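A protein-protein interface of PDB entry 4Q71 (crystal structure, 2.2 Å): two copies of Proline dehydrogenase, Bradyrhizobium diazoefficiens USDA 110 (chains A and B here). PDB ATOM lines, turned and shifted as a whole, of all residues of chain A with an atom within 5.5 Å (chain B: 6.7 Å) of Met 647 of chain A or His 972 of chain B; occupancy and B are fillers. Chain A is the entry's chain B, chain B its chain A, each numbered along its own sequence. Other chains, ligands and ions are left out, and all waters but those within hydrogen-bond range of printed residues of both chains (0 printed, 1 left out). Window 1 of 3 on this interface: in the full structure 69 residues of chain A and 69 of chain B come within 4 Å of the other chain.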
ATOM      1  N   LEU A 628     -26.205 -14.343 -13.933  1.00  0.00           N
ATOM      2  CA  LEU A 628     -26.394 -13.212 -14.840  1.00  0.00           C
ATOM      3  C   LEU A 628     -26.206 -11.839 -14.177  1.00  0.00           C
ATOM      4  O   LEU A 628     -25.561 -10.949 -14.735  1.00  0.00           O
ATOM      5  CB  LEU A 628     -27.785 -13.301 -15.482  1.00  0.00           C
ATOM      6  CG  LEU A 628     -28.080 -12.356 -16.644  1.00  0.00           C
ATOM      7  CD1 LEU A 628     -26.971 -12.476 -17.673  1.00  0.00           C
ATOM      8  CD2 LEU A 628     -29.436 -12.687 -17.286  1.00  0.00           C
ATOM      9  N   PHE A 629     -26.783 -11.653 -12.999  1.00  0.00           N
ATOM     10  CA  PHE A 629     -26.767 -10.330 -12.373  1.00  0.00           C
ATOM     11  C   PHE A 629     -25.818 -10.263 -11.166  1.00  0.00           C
ATOM     12  O   PHE A 629     -25.626  -9.202 -10.581  1.00  0.00           O
ATOM     13  CB  PHE A 629     -28.188  -9.944 -11.949  1.00  0.00           C
ATOM     14  CG  PHE A 629     -29.233 -10.202 -13.014  1.00  0.00           C
ATOM     15  CD1 PHE A 629     -30.255 -11.126 -12.797  1.00  0.00           C
ATOM     16  CD2 PHE A 629     -29.191  -9.525 -14.234  1.00  0.00           C
ATOM     17  CE1 PHE A 629     -31.220 -11.374 -13.778  1.00  0.00           C
ATOM     18  CE2 PHE A 629     -30.151  -9.757 -15.220  1.00  0.00           C
ATOM     19  CZ  PHE A 629     -31.170 -10.692 -14.994  1.00  0.00           C
ATOM     20  N   LEU A 645     -19.412  -4.990 -18.364  1.00  0.00           N
ATOM     21  CA  LEU A 645     -20.793  -5.085 -18.800  1.00  0.00           C
ATOM     22  C   LEU A 645     -21.632  -5.570 -17.634  1.00  0.00           C
ATOM     23  O   LEU A 645     -21.335  -6.599 -17.015  1.00  0.00           O
ATOM     24  CB  LEU A 645     -20.913  -6.053 -19.996  1.00  0.00           C
ATOM     25  CG  LEU A 645     -22.284  -6.208 -20.659  1.00  0.00           C
ATOM     26  CD1 LEU A 645     -22.766  -4.885 -21.250  1.00  0.00           C
ATOM     27  CD2 LEU A 645     -22.216  -7.276 -21.748  1.00  0.00           C
ATOM     28  N   THR A 646     -22.679  -4.821 -17.326  1.00  0.00           N
ATOM     29  CA  THR A 646     -23.604  -5.213 -16.277  1.00  0.00           C
ATOM     30  C   THR A 646     -25.010  -5.275 -16.852  1.00  0.00           C
ATOM     31  O   THR A 646     -25.268  -4.825 -17.972  1.00  0.00           O
ATOM     32  CB  THR A 646     -23.598  -4.227 -15.096  1.00  0.00           C
ATOM     33  OG1 THR A 646     -23.778  -2.897 -15.590  1.00  0.00           O
ATOM     34  CG2 THR A 646     -22.289  -4.306 -14.336  1.00  0.00           C
ATOM     35  N   MET A 647     -25.919  -5.830 -16.075  1.00  0.00           N
ATOM     36  CA  MET A 647     -27.313  -5.909 -16.472  1.00  0.00           C
ATOM     37  C   MET A 647     -28.165  -5.369 -15.351  1.00  0.00           C
ATOM     38  O   MET A 647     -28.077  -5.844 -14.218  1.00  0.00           O
ATOM     39  CB  MET A 647     -27.703  -7.357 -16.726  1.00  0.00           C
ATOM     40  CG  MET A 647     -26.710  -8.097 -17.567  1.00  0.00           C
ATOM     41  SD  MET A 647     -27.290  -8.087 -19.250  1.00  0.00           S
ATOM     42  CE  MET A 647     -28.561  -9.309 -19.065  1.00  0.00           C
ATOM     43  N   ARG A 648     -29.008  -4.395 -15.669  1.00  0.00           N
ATOM     44  CA  ARG A 648     -29.789  -3.723 -14.649  1.00  0.00           C
ATOM     45  C   ARG A 648     -31.279  -3.922 -14.903  1.00  0.00           C
ATOM     46  O   ARG A 648     -31.693  -4.140 -16.044  1.00  0.00           O
ATOM     47  CB  ARG A 648     -29.487  -2.227 -14.676  1.00  0.00           C
ATOM     48  CG  ARG A 648     -28.029  -1.847 -14.542  1.00  0.00           C
ATOM     49  CD  ARG A 648     -27.894  -0.328 -14.678  1.00  0.00           C
ATOM     50  NE  ARG A 648     -28.649   0.348 -13.624  1.00  0.00           N
ATOM     51  CZ  ARG A 648     -28.199   1.350 -12.870  1.00  0.00           C
ATOM     52  NH1 ARG A 648     -26.973   1.855 -13.056  1.00  0.00           N
ATOM     53  NH2 ARG A 648     -28.994   1.860 -11.932  1.00  0.00           N
ATOM     54  N   GLY A 649     -32.080  -3.824 -13.841  1.00  0.00           N
ATOM     55  CA  GLY A 649     -33.528  -3.810 -13.969  1.00  0.00           C
ATOM     56  C   GLY A 649     -33.968  -2.720 -14.931  1.00  0.00           C
ATOM     57  O   GLY A 649     -33.270  -1.715 -15.094  1.00  0.00           O
ATOM     58  N   ALA A 676     -34.559  -9.962 -12.117  1.00  0.00           N
ATOM     59  CA  ALA A 676     -33.822  -9.075 -13.006  1.00  0.00           C
ATOM     60  C   ALA A 676     -33.681  -7.673 -12.418  1.00  0.00           C
ATOM     61  O   ALA A 676     -32.965  -6.822 -12.971  1.00  0.00           O
ATOM     62  CB  ALA A 676     -34.490  -9.017 -14.354  1.00  0.00           C
ATOM     63  N   ALA A 975     -32.458 -12.287 -19.140  1.00  0.00           N
ATOM     64  CA  ALA A 975     -31.809 -11.173 -19.835  1.00  0.00           C
ATOM     65  C   ALA A 975     -32.816 -10.242 -20.500  1.00  0.00           C
ATOM     66  O   ALA A 975     -32.595  -9.033 -20.569  1.00  0.00           O
ATOM     67  CB  ALA A 975     -30.811 -11.690 -20.872  1.00  0.00           C
ATOM     68  N   ALA A 978     -34.051  -7.347 -18.510  1.00  0.00           N
ATOM     69  CA  ALA A 978     -33.024  -6.421 -18.048  1.00  0.00           C
ATOM     70  C   ALA A 978     -32.486  -5.579 -19.187  1.00  0.00           C
ATOM     71  O   ALA A 978     -32.833  -5.793 -20.349  1.00  0.00           O
ATOM     72  CB  ALA A 978     -31.875  -7.176 -17.343  1.00  0.00           C
ATOM     73  N   THR A 979     -31.648  -4.609 -18.840  1.00  0.00           N
ATOM     74  CA  THR A 979     -31.017  -3.759 -19.831  1.00  0.00           C
ATOM     75  C   THR A 979     -29.520  -3.794 -19.570  1.00  0.00           C
ATOM     76  O   THR A 979     -29.104  -3.946 -18.432  1.00  0.00           O
ATOM     77  CB  THR A 979     -31.612  -2.315 -19.823  1.00  0.00           C
ATOM     78  OG1 THR A 979     -31.138  -1.585 -20.957  1.00  0.00           O
ATOM     79  CG2 THR A 979     -31.223  -1.562 -18.561  1.00  0.00           C
ATOM     80  N   GLU A 980     -28.714  -3.734 -20.625  1.00  0.00           N
ATOM     81  CA  GLU A 980     -27.265  -3.776 -20.481  1.00  0.00           C
ATOM     82  C   GLU A 980     -26.713  -2.386 -20.165  1.00  0.00           C
ATOM     83  O   GLU A 980     -27.261  -1.368 -20.598  1.00  0.00           O
ATOM     84  CB  GLU A 980     -26.607  -4.268 -21.764  1.00  0.00           C
ATOM     85  CG  GLU A 980     -26.825  -5.714 -22.107  1.00  0.00           C
ATOM     86  CD  GLU A 980     -26.517  -5.990 -23.572  1.00  0.00           C
ATOM     87  OE1 GLU A 980     -25.352  -6.320 -23.888  1.00  0.00           O
ATOM     88  OE2 GLU A 980     -27.430  -5.821 -24.415  1.00  0.00           O
ATOM     89  N   GLN A 981     -25.615  -2.352 -19.428  1.00  0.00           N
ATOM     90  CA  GLN A 981     -24.885  -1.122 -19.220  1.00  0.00           C
ATOM     91  C   GLN A 981     -23.385  -1.371 -19.271  1.00  0.00           C
ATOM     92  O   GLN A 981     -22.856  -2.230 -18.573  1.00  0.00           O
ATOM     93  CB  GLN A 981     -25.309  -0.462 -17.902  1.00  0.00           C
ATOM     94  CG  GLN A 981     -24.463   0.735 -17.495  1.00  0.00           C
ATOM     95  CD  GLN A 981     -25.062   1.494 -16.313  1.00  0.00           C
ATOM     96  OE1 GLN A 981     -24.776   1.190 -15.156  1.00  0.00           O
ATOM     97  NE2 GLN A 981     -25.899   2.490 -16.609  1.00  0.00           N
ATOM     98  N   TYR B 620     -16.243 -10.494 -34.853  1.00  0.00           N
ATOM     99  CA  TYR B 620     -16.840 -10.669 -33.537  1.00  0.00           C
ATOM    100  C   TYR B 620     -18.139 -11.474 -33.590  1.00  0.00           C
ATOM    101  O   TYR B 620     -18.350 -12.409 -32.799  1.00  0.00           O
ATOM    102  CB  TYR B 620     -17.119  -9.319 -32.902  1.00  0.00           C
ATOM    103  CG  TYR B 620     -17.781  -9.436 -31.551  1.00  0.00           C
ATOM    104  CD1 TYR B 620     -17.045  -9.824 -30.430  1.00  0.00           C
ATOM    105  CD2 TYR B 620     -19.138  -9.168 -31.390  1.00  0.00           C
ATOM    106  CE1 TYR B 620     -17.646  -9.940 -29.172  1.00  0.00           C
ATOM    107  CE2 TYR B 620     -19.745  -9.266 -30.131  1.00  0.00           C
ATOM    108  CZ  TYR B 620     -18.984  -9.659 -29.034  1.00  0.00           C
ATOM    109  OH  TYR B 620     -19.575  -9.782 -27.803  1.00  0.00           O
ATOM    110  N   GLN B 624     -18.779 -15.050 -31.815  1.00  0.00           N
ATOM    111  CA  GLN B 624     -19.951 -15.245 -30.960  1.00  0.00           C
ATOM    112  C   GLN B 624     -20.938 -16.189 -31.630  1.00  0.00           C
ATOM    113  O   GLN B 624     -21.607 -16.974 -30.959  1.00  0.00           O
ATOM    114  CB  GLN B 624     -20.636 -13.911 -30.644  1.00  0.00           C
ATOM    115  CG  GLN B 624     -19.761 -12.937 -29.889  1.00  0.00           C
ATOM    116  CD  GLN B 624     -19.492 -13.402 -28.479  1.00  0.00           C
ATOM    117  OE1 GLN B 624     -18.342 -13.486 -28.044  1.00  0.00           O
ATOM    118  NE2 GLN B 624     -20.557 -13.699 -27.748  1.00  0.00           N
ATOM    119  N   PRO B 966     -30.978  -5.633 -27.902  1.00  0.00           N
ATOM    120  CA  PRO B 966     -29.736  -5.736 -27.127  1.00  0.00           C
ATOM    121  C   PRO B 966     -28.625  -4.863 -27.749  1.00  0.00           C
ATOM    122  O   PRO B 966     -28.824  -4.256 -28.810  1.00  0.00           O
ATOM    123  CB  PRO B 966     -29.400  -7.230 -27.214  1.00  0.00           C
ATOM    124  CG  PRO B 966     -29.989  -7.665 -28.528  1.00  0.00           C
ATOM    125  CD  PRO B 966     -31.247  -6.846 -28.700  1.00  0.00           C
ATOM    126  N   LYS B 967     -27.488  -4.775 -27.069  1.00  0.00           N
ATOM    127  CA  LYS B 967     -26.372  -3.948 -27.517  1.00  0.00           C
ATOM    128  C   LYS B 967     -25.605  -4.565 -28.689  1.00  0.00           C
ATOM    129  O   LYS B 967     -25.125  -5.694 -28.599  1.00  0.00           O
ATOM    130  CB  LYS B 967     -25.392  -3.718 -26.360  1.00  0.00           C
ATOM    131  CG  LYS B 967     -25.821  -2.711 -25.300  1.00  0.00           C
ATOM    132  CD  LYS B 967     -24.777  -2.703 -24.179  1.00  0.00           C
ATOM    133  CE  LYS B 967     -24.893  -1.501 -23.236  1.00  0.00           C
ATOM    134  NZ  LYS B 967     -24.336  -0.258 -23.833  1.00  0.00           N
ATOM    135  N   GLY B 969     -22.414  -5.294 -30.955  1.00  0.00           N
ATOM    136  CA  GLY B 969     -21.019  -5.499 -30.599  1.00  0.00           C
ATOM    137  C   GLY B 969     -20.824  -6.055 -29.197  1.00  0.00           C
ATOM    138  O   GLY B 969     -19.730  -5.946 -28.630  1.00  0.00           O
ATOM    139  N   GLY B 970     -21.883  -6.649 -28.641  1.00  0.00           N
ATOM    140  CA  GLY B 970     -21.831  -7.269 -27.324  1.00  0.00           C
ATOM    141  C   GLY B 970     -22.374  -8.696 -27.338  1.00  0.00           C
ATOM    142  O   GLY B 970     -22.879  -9.159 -28.355  1.00  0.00           O
ATOM    143  N   PRO B 971     -22.285  -9.399 -26.203  1.00  0.00           N
ATOM    144  CA  PRO B 971     -22.582 -10.843 -26.184  1.00  0.00           C
ATOM    145  C   PRO B 971     -24.056 -11.228 -26.125  1.00  0.00           C
ATOM    146  O   PRO B 971     -24.337 -12.431 -26.058  1.00  0.00           O
ATOM    147  CB  PRO B 971     -21.861 -11.333 -24.915  1.00  0.00           C
ATOM    148  CG  PRO B 971     -21.850 -10.123 -24.000  1.00  0.00           C
ATOM    149  CD  PRO B 971     -21.699  -8.924 -24.935  1.00  0.00           C
ATOM    150  N   HIS B 972     -24.971 -10.261 -26.162  1.00  0.00           N
ATOM    151  CA  HIS B 972     -26.406 -10.579 -26.108  1.00  0.00           C
ATOM    152  C   HIS B 972     -27.122 -10.263 -27.422  1.00  0.00           C
ATOM    153  O   HIS B 972     -28.328 -10.449 -27.543  1.00  0.00           O
ATOM    154  CB  HIS B 972     -27.084  -9.823 -24.961  1.00  0.00           C
ATOM    155  CG  HIS B 972     -26.502 -10.134 -23.619  1.00  0.00           C
ATOM    156  ND1 HIS B 972     -26.978 -11.150 -22.819  1.00  0.00           N
ATOM    157  CD2 HIS B 972     -25.463  -9.580 -22.948  1.00  0.00           C
ATOM    158  CE1 HIS B 972     -26.270 -11.198 -21.704  1.00  0.00           C
ATOM    159  NE2 HIS B 972     -25.340 -10.260 -21.760  1.00  0.00           N
ATOM    160  N   TYR B 973     -26.364  -9.819 -28.413  1.00  0.00           N
ATOM    161  CA  TYR B 973     -26.950  -9.316 -29.656  1.00  0.00           C
ATOM    162  C   TYR B 973     -27.476 -10.423 -30.558  1.00  0.00           C
ATOM    163  O   TYR B 973     -28.617 -10.370 -30.993  1.00  0.00           O
ATOM    164  CB  TYR B 973     -25.911  -8.497 -30.399  1.00  0.00           C
ATOM    165  CG  TYR B 973     -26.428  -7.577 -31.478  1.00  0.00           C
ATOM    166  CD1 TYR B 973     -27.295  -6.528 -31.183  1.00  0.00           C
ATOM    167  CD2 TYR B 973     -25.992  -7.720 -32.792  1.00  0.00           C
ATOM    168  CE1 TYR B 973     -27.734  -5.663 -32.187  1.00  0.00           C
ATOM    169  CE2 TYR B 973     -26.412  -6.862 -33.791  1.00  0.00           C
ATOM    170  CZ  TYR B 973     -27.286  -5.845 -33.488  1.00  0.00           C
ATOM    171  OH  TYR B 973     -27.691  -5.012 -34.493  1.00  0.00           O
ATOM    172  N   LEU B 974     -26.623 -11.404 -30.849  1.00  0.00           N
ATOM    173  CA  LEU B 974     -26.933 -12.459 -31.813  1.00  0.00           C
ATOM    174  C   LEU B 974     -28.184 -13.271 -31.462  1.00  0.00           C
ATOM    175  O   LEU B 974     -28.985 -13.589 -32.344  1.00  0.00           O
ATOM    176  CB  LEU B 974     -25.723 -13.382 -32.011  1.00  0.00           C
ATOM    177  CG  LEU B 974     -24.542 -12.778 -32.795  1.00  0.00           C
ATOM    178  CD1 LEU B 974     -23.449 -13.797 -33.078  1.00  0.00           C
ATOM    179  CD2 LEU B 974     -25.011 -12.177 -34.108  1.00  0.00           C
ATOM    180  N   ALA B 975     -28.363 -13.587 -30.183  1.00  0.00           N
ATOM    181  CA  ALA B 975     -29.503 -14.397 -29.748  1.00  0.00           C
ATOM    182  C   ALA B 975     -30.852 -13.776 -30.127  1.00  0.00           C
ATOM    183  O   ALA B 975     -31.817 -14.488 -30.406  1.00  0.00           O
ATOM    184  CB  ALA B 975     -29.435 -14.635 -28.252  1.00  0.00           C
ATOM    185  N   ARG B 976     -30.909 -12.447 -30.138  1.00  0.00           N
ATOM    186  CA  ARG B 976     -32.150 -11.748 -30.454  1.00  0.00           C
ATOM    187  C   ARG B 976     -32.599 -12.017 -31.893  1.00  0.00           C
ATOM    188  O   ARG B 976     -33.783 -11.909 -32.203  1.00  0.00           O
ATOM    189  CB  ARG B 976     -31.986 -10.247 -30.231  1.00  0.00           C
ATOM    190  CG  ARG B 976     -33.298  -9.486 -30.177  1.00  0.00           C
ATOM    191  CD  ARG B 976     -33.926  -9.613 -28.800  1.00  0.00           C
ATOM    192  NE  ARG B 976     -35.243  -8.995 -28.758  1.00  0.00           N
ATOM    193  CZ  ARG B 976     -36.368  -9.628 -29.075  1.00  0.00           C
ATOM    194  NH1 ARG B 976     -36.329 -10.898 -29.463  1.00  0.00           N
ATOM    195  NH2 ARG B 976     -37.531  -8.996 -29.009  1.00  0.00           N
ATOM    196  N   PHE B 977     -31.647 -12.353 -32.764  1.00  0.00           N
ATOM    197  CA  PHE B 977     -31.947 -12.618 -34.169  1.00  0.00           C
ATOM    198  C   PHE B 977     -32.371 -14.059 -34.391  1.00  0.00           C
ATOM    199  O   PHE B 977     -32.623 -14.480 -35.533  1.00  0.00           O
ATOM    200  CB  PHE B 977     -30.731 -12.323 -35.046  1.00  0.00           C
ATOM    201  CG  PHE B 977     -30.357 -10.867 -35.100  1.00  0.00           C
ATOM    202  CD1 PHE B 977     -29.581 -10.293 -34.091  1.00  0.00           C
ATOM    203  CD2 PHE B 977     -30.782 -10.063 -36.157  1.00  0.00           C
ATOM    204  CE1 PHE B 977     -29.229  -8.955 -34.141  1.00  0.00           C
ATOM    205  CE2 PHE B 977     -30.435  -8.712 -36.215  1.00  0.00           C
ATOM    206  CZ  PHE B 977     -29.653  -8.162 -35.199  1.00  0.00           C
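The backbone NH (N) of Thr 646 of chain A lies within hydrogen-bond range of the backbone carbonyl oxygen (O) of Gln 981 of chain A (2.9 Å). The guanidinium group (NH1) of Arg 648 of chain A lies within hydrogen-bond range of the side-chain amide oxygen (OE1) of Gln 981 of chain A (3.1 Å).
Printed residues of chain B that touch a printed residue of chain A: Pro 966, Lys 967, Pro 971 and His 972. Of the 13 printed residues of chain A, 4 touch a printed residue of chain B. Printed residues of chain A that touch a printed residue of chain B: Leu 645, Met 647, Glu 980 and Gln 981. Among the printed residues, no Asp or Glu carboxylate lies within 4 Å of a Lys or Arg side-chain nitrogen of the other chain.
Leu 645 of chain A touches Pro 971 of chain B (CD2 to CD, 3.6 Å). His 972 of chain B touches Met 647 of chain A (NE2 to SD, 3.9 Å). Pro 966 of chain B touches Glu 980 of chain A. CD2 of His 972 of chain B touches OE1 of Glu 980 of chain A, at 3.4 Å. Gln 981 of chain A touches Lys 967 of chain B (N to CE, 3.97 Å).
OE2 of Glu 980 of chain A is in hydrogen-bond range of N of Lys 967 of chain B (2.9 Å).
1 position is printed for both chains.
Met 647 of chain A touches one residue of chain B. Of chain A, only Met 647 (3.9 Å) and Glu 980 (3.4 Å) come within 4 Å of His 972 of chain B. Printed residues of chain B within 4 Å of Glu 980 of chain A: Pro 966 (3.6 Å), Lys 967 (2.9 Å) and His 972 (3.4 Å). Of the printed residues of chain A, Lys 967 of chain B touches Glu 980 (2.9 Å) and Gln 981 (3.97 Å). The nearest residue of chain A that does not touch His 972 of chain B is Leu 645 of chain A (4.2 Å). The nearest printed residue of chain B that does not touch Gln 981 of chain A is His 972 of chain B (8.0 Å).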
